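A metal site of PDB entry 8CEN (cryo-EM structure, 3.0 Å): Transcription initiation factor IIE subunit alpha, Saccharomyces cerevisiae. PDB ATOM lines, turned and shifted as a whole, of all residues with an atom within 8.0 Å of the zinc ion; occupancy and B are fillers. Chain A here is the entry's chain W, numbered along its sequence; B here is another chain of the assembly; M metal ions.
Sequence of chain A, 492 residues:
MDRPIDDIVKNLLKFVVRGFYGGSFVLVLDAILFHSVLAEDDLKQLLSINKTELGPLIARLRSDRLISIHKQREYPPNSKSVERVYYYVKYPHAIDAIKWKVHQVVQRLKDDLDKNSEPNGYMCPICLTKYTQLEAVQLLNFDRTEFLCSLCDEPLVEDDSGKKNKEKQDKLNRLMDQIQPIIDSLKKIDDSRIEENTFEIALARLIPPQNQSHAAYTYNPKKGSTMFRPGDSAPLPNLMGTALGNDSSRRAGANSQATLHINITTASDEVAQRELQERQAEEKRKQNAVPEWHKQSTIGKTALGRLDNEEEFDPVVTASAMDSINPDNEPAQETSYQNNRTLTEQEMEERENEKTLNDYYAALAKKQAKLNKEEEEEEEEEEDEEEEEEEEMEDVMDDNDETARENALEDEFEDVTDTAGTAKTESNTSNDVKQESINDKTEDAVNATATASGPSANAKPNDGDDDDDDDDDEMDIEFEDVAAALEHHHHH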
ATOM      1  N   MET A 123     -24.874  -8.011  34.070  1.00  0.00           N
ATOM      2  CA  MET A 123     -25.704  -7.449  33.016  1.00  0.00           C
ATOM      3  C   MET A 123     -25.590  -8.332  31.773  1.00  0.00           C
ATOM      4  O   MET A 123     -24.551  -8.951  31.531  1.00  0.00           O
ATOM      5  CB  MET A 123     -25.327  -5.981  32.721  1.00  0.00           C
ATOM      6  CG  MET A 123     -23.899  -5.712  32.228  1.00  0.00           C
ATOM      7  SD  MET A 123     -23.529  -6.031  30.480  1.00  0.00           S
ATOM      8  CE  MET A 123     -24.433  -4.702  29.701  1.00  0.00           C
ATOM      9  N   CYS A 124     -26.677  -8.392  31.002  1.00  0.00           N
ATOM     10  CA  CYS A 124     -26.705  -9.237  29.812  1.00  0.00           C
ATOM     11  C   CYS A 124     -26.380  -8.389  28.589  1.00  0.00           C
ATOM     12  O   CYS A 124     -27.124  -7.443  28.291  1.00  0.00           O
ATOM     13  CB  CYS A 124     -28.070  -9.892  29.644  1.00  0.00           C
ATOM     14  SG  CYS A 124     -28.148 -11.082  28.288  1.00  0.00           S
ATOM     15  N   PRO A 125     -25.283  -8.667  27.872  1.00  0.00           N
ATOM     16  CA  PRO A 125     -24.929  -7.837  26.713  1.00  0.00           C
ATOM     17  C   PRO A 125     -25.915  -7.927  25.561  1.00  0.00           C
ATOM     18  O   PRO A 125     -26.024  -6.961  24.795  1.00  0.00           O
ATOM     19  CB  PRO A 125     -23.544  -8.356  26.325  1.00  0.00           C
ATOM     20  CG  PRO A 125     -23.506  -9.761  26.831  1.00  0.00           C
ATOM     21  CD  PRO A 125     -24.294  -9.739  28.112  1.00  0.00           C
ATOM     22  N   ILE A 126     -26.614  -9.046  25.417  1.00  0.00           N
ATOM     23  CA  ILE A 126     -27.535  -9.202  24.284  1.00  0.00           C
ATOM     24  C   ILE A 126     -28.772  -8.318  24.470  1.00  0.00           C
ATOM     25  O   ILE A 126     -29.160  -7.576  23.563  1.00  0.00           O
ATOM     26  CB  ILE A 126     -27.925 -10.679  24.103  1.00  0.00           C
ATOM     27  CG1 ILE A 126     -26.675 -11.523  23.837  1.00  0.00           C
ATOM     28  CG2 ILE A 126     -28.939 -10.828  22.981  1.00  0.00           C
ATOM     29  CD1 ILE A 126     -26.969 -12.936  23.372  1.00  0.00           C
ATOM     30  N   CYS A 127     -29.388  -8.382  25.645  1.00  0.00           N
ATOM     31  CA  CYS A 127     -30.617  -7.628  25.899  1.00  0.00           C
ATOM     32  C   CYS A 127     -30.370  -6.279  26.558  1.00  0.00           C
ATOM     33  O   CYS A 127     -31.319  -5.502  26.696  1.00  0.00           O
ATOM     34  CB  CYS A 127     -31.573  -8.458  26.761  1.00  0.00           C
ATOM     35  SG  CYS A 127     -31.033  -8.720  28.466  1.00  0.00           S
ATOM     36  N   LEU A 128     -29.118  -5.987  26.941  1.00  0.00           N
ATOM     37  CA  LEU A 128     -28.719  -4.711  27.554  1.00  0.00           C
ATOM     38  C   LEU A 128     -29.535  -4.395  28.815  1.00  0.00           C
ATOM     39  O   LEU A 128     -29.924  -3.242  29.048  1.00  0.00           O
ATOM     40  CB  LEU A 128     -28.802  -3.553  26.547  1.00  0.00           C
ATOM     41  CG  LEU A 128     -27.822  -3.626  25.371  1.00  0.00           C
ATOM     42  CD1 LEU A 128     -27.978  -2.411  24.468  1.00  0.00           C
ATOM     43  CD2 LEU A 128     -26.394  -3.752  25.872  1.00  0.00           C
ATOM     44  N   THR A 129     -29.782  -5.415  29.626  1.00  0.00           N
ATOM     45  CA  THR A 129     -30.502  -5.262  30.875  1.00  0.00           C
ATOM     46  C   THR A 129     -29.633  -5.755  32.035  1.00  0.00           C
ATOM     47  O   THR A 129     -28.904  -6.732  31.894  1.00  0.00           O
ATOM     48  CB  THR A 129     -31.830  -6.033  30.873  1.00  0.00           C
ATOM     49  OG1 THR A 129     -31.580  -7.434  30.706  1.00  0.00           O
ATOM     50  CG2 THR A 129     -32.739  -5.536  29.751  1.00  0.00           C
ATOM     51  N   LYS A 130     -29.743  -5.069  33.170  1.00  0.00           N
ATOM     52  CA  LYS A 130     -28.972  -5.417  34.354  1.00  0.00           C
ATOM     53  C   LYS A 130     -29.732  -6.427  35.214  1.00  0.00           C
ATOM     54  O   LYS A 130     -30.957  -6.531  35.166  1.00  0.00           O
ATOM     55  CB  LYS A 130     -28.656  -4.165  35.172  1.00  0.00           C
ATOM     56  CG  LYS A 130     -29.876  -3.473  35.751  1.00  0.00           C
ATOM     57  CD  LYS A 130     -29.486  -2.252  36.569  1.00  0.00           C
ATOM     58  CE  LYS A 130     -29.029  -1.117  35.674  1.00  0.00           C
ATOM     59  NZ  LYS A 130     -28.767   0.125  36.455  1.00  0.00           N
ATOM     60  N   TYR A 131     -28.973  -7.186  35.996  1.00  0.00           N
ATOM     61  CA  TYR A 131     -29.520  -8.179  36.911  1.00  0.00           C
ATOM     62  C   TYR A 131     -28.560  -8.237  38.093  1.00  0.00           C
ATOM     63  O   TYR A 131     -27.416  -8.676  37.937  1.00  0.00           O
ATOM     64  CB  TYR A 131     -29.635  -9.549  36.252  1.00  0.00           C
ATOM     65  CG  TYR A 131     -30.788  -9.699  35.287  1.00  0.00           C
ATOM     66  CD1 TYR A 131     -32.054 -10.041  35.750  1.00  0.00           C
ATOM     67  CD2 TYR A 131     -30.612  -9.516  33.926  1.00  0.00           C
ATOM     68  CE1 TYR A 131     -33.114 -10.186  34.868  1.00  0.00           C
ATOM     69  CE2 TYR A 131     -31.664  -9.665  33.040  1.00  0.00           C
ATOM     70  CZ  TYR A 131     -32.916  -9.998  33.517  1.00  0.00           C
ATOM     71  OH  TYR A 131     -33.966 -10.134  32.641  1.00  0.00           O
ATOM     72  N   LEU A 148     -27.814 -17.586  33.615  1.00  0.00           N
ATOM     73  CA  LEU A 148     -28.364 -17.481  32.272  1.00  0.00           C
ATOM     74  C   LEU A 148     -29.493 -16.456  32.272  1.00  0.00           C
ATOM     75  O   LEU A 148     -30.304 -16.416  33.202  1.00  0.00           O
ATOM     76  CB  LEU A 148     -28.878 -18.826  31.767  1.00  0.00           C
ATOM     77  CG  LEU A 148     -27.902 -19.825  31.119  1.00  0.00           C
ATOM     78  CD1 LEU A 148     -27.300 -19.238  29.843  1.00  0.00           C
ATOM     79  CD2 LEU A 148     -26.793 -20.288  32.046  1.00  0.00           C
ATOM     80  N   CYS A 149     -29.543 -15.633  31.224  1.00  0.00           N
ATOM     81  CA  CYS A 149     -30.541 -14.575  31.131  1.00  0.00           C
ATOM     82  C   CYS A 149     -31.934 -15.159  30.979  1.00  0.00           C
ATOM     83  O   CYS A 149     -32.132 -16.240  30.405  1.00  0.00           O
ATOM     84  CB  CYS A 149     -30.227 -13.643  29.960  1.00  0.00           C
ATOM     85  SG  CYS A 149     -31.490 -12.400  29.607  1.00  0.00           S
ATOM     86  N   SER A 150     -32.925 -14.437  31.521  1.00  0.00           N
ATOM     87  CA  SER A 150     -34.303 -14.919  31.489  1.00  0.00           C
ATOM     88  C   SER A 150     -34.885 -14.895  30.083  1.00  0.00           C
ATOM     89  O   SER A 150     -35.734 -15.726  29.748  1.00  0.00           O
ATOM     90  CB  SER A 150     -35.169 -14.084  32.446  1.00  0.00           C
ATOM     91  OG  SER A 150     -35.256 -12.734  31.994  1.00  0.00           O
ATOM     92  N   LEU A 151     -34.446 -13.948  29.248  1.00  0.00           N
ATOM     93  CA  LEU A 151     -34.946 -13.824  27.885  1.00  0.00           C
ATOM     94  C   LEU A 151     -33.932 -14.358  26.868  1.00  0.00           C
ATOM     95  O   LEU A 151     -34.271 -15.212  26.049  1.00  0.00           O
ATOM     96  CB  LEU A 151     -35.299 -12.353  27.610  1.00  0.00           C
ATOM     97  CG  LEU A 151     -36.003 -11.893  26.324  1.00  0.00           C
ATOM     98  CD1 LEU A 151     -36.783 -10.613  26.611  1.00  0.00           C
ATOM     99  CD2 LEU A 151     -35.051 -11.640  25.162  1.00  0.00           C
ATOM    100  N   CYS A 152     -32.693 -13.860  26.915  1.00  0.00           N
ATOM    101  CA  CYS A 152     -31.695 -14.215  25.919  1.00  0.00           C
ATOM    102  C   CYS A 152     -31.107 -15.601  26.117  1.00  0.00           C
ATOM    103  O   CYS A 152     -30.576 -16.169  25.154  1.00  0.00           O
ATOM    104  CB  CYS A 152     -30.570 -13.173  25.916  1.00  0.00           C
ATOM    105  SG  CYS A 152     -31.136 -11.464  25.924  1.00  0.00           S
ATOM    106  N   ASP A 153     -31.202 -16.155  27.336  1.00  0.00           N
ATOM    107  CA  ASP A 153     -30.565 -17.424  27.716  1.00  0.00           C
ATOM    108  C   ASP A 153     -29.056 -17.392  27.422  1.00  0.00           C
ATOM    109  O   ASP A 153     -28.498 -18.309  26.823  1.00  0.00           O
ATOM    110  CB  ASP A 153     -31.236 -18.615  27.048  1.00  0.00           C
ATOM    111  CG  ASP A 153     -32.678 -18.794  27.478  1.00  0.00           C
ATOM    112  OD1 ASP A 153     -33.188 -17.917  28.213  1.00  0.00           O
ATOM    113  OD2 ASP A 153     -33.299 -19.800  27.084  1.00  0.00           O
ATOM    114  N   GLU A 154     -28.418 -16.314  27.864  1.00  0.00           N
ATOM    115  CA  GLU A 154     -27.005 -16.055  27.652  1.00  0.00           C
ATOM    116  C   GLU A 154     -26.287 -15.943  28.983  1.00  0.00           C
ATOM    117  O   GLU A 154     -26.858 -15.425  29.948  1.00  0.00           O
ATOM    118  CB  GLU A 154     -26.817 -14.758  26.829  1.00  0.00           C
ATOM    119  CG  GLU A 154     -25.404 -14.481  26.346  1.00  0.00           C
ATOM    120  CD  GLU A 154     -24.716 -13.421  27.180  1.00  0.00           C
ATOM    121  OE1 GLU A 154     -25.362 -12.855  28.086  1.00  0.00           O
ATOM    122  OE2 GLU A 154     -23.520 -13.143  26.915  1.00  0.00           O
ATOM    123  N   PRO A 155     -25.060 -16.456  29.094  1.00  0.00           N
ATOM    124  CA  PRO A 155     -24.306 -16.343  30.355  1.00  0.00           C
ATOM    125  C   PRO A 155     -24.029 -14.890  30.736  1.00  0.00           C
ATOM    126  O   PRO A 155     -23.490 -14.116  29.946  1.00  0.00           O
ATOM    127  CB  PRO A 155     -23.007 -17.101  30.070  1.00  0.00           C
ATOM    128  CG  PRO A 155     -23.405 -18.108  29.042  1.00  0.00           C
ATOM    129  CD  PRO A 155     -24.426 -17.420  28.176  1.00  0.00           C
ATOM    130  N   LEU A 156     -24.413 -14.535  31.963  1.00  0.00           N
ATOM    131  CA  LEU A 156     -24.306 -13.166  32.439  1.00  0.00           C
ATOM    132  C   LEU A 156     -22.839 -12.763  32.604  1.00  0.00           C
ATOM    133  O   LEU A 156     -22.016 -13.552  33.076  1.00  0.00           O
ATOM    134  CB  LEU A 156     -25.039 -13.018  33.779  1.00  0.00           C
ATOM    135  CG  LEU A 156     -26.513 -12.593  33.834  1.00  0.00           C
ATOM    136  CD1 LEU A 156     -26.678 -11.128  33.489  1.00  0.00           C
ATOM    137  CD2 LEU A 156     -27.405 -13.451  32.949  1.00  0.00           C
ATOM    138  N   GLY B  15     -29.872  -7.041  20.172  1.00  0.00           N
ATOM    139  CA  GLY B  15     -31.127  -6.739  20.822  1.00  0.00           C
ATOM    140  C   GLY B  15     -31.879  -7.981  21.232  1.00  0.00           C
ATOM    141  O   GLY B  15     -31.482  -9.115  20.910  1.00  0.00           O
ATOM    142  N   PRO B  16     -32.982  -7.811  21.953  1.00  0.00           N
ATOM    143  CA  PRO B  16     -33.805  -8.965  22.335  1.00  0.00           C
ATOM    144  C   PRO B  16     -34.494  -9.578  21.132  1.00  0.00           C
ATOM    145  O   PRO B  16     -34.738  -8.909  20.124  1.00  0.00           O
ATOM    146  CB  PRO B  16     -34.824  -8.382  23.320  1.00  0.00           C
ATOM    147  CG  PRO B  16     -34.690  -6.909  23.259  1.00  0.00           C
ATOM    148  CD  PRO B  16     -33.469  -6.536  22.506  1.00  0.00           C
HETATM  149 ZN    ZN M   1     -30.464 -10.947  28.094  1.00  0.00          ZN
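The side-chain sulfur of Cys 149 sits close to the backbone NH of Leu 151 (3.4 Å).
The backbone NH (N) of Cys 149 lies within hydrogen-bond range of the backbone carbonyl oxygen (O) of Glu 154 (3.0 Å).
OG1 of Thr 129 lies close to SG of Cys 127 (2.6 Å).
The backbone NH (N) of Cys 124 is in hydrogen-bond range of the backbone carbonyl oxygen (O) of Thr 129, 2.9 Å away.
The side-chain carboxylate (OE1) of Glu 154 sits close to the side-chain sulfur (SG) of Cys 124.
The zinc ion is bound by SG of Cys 127, SG of Cys 124, SG of Cys 152 and SG of Cys 149.
The zinc ion has four donor atoms within binding distance.
Four residues have an atom within 4 Å of the zinc ion: Cys 124, Cys 127, Cys 149 and Cys 152.
The nearest printed residue that does not touch the zinc ion is Thr 129 (4.5 Å).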
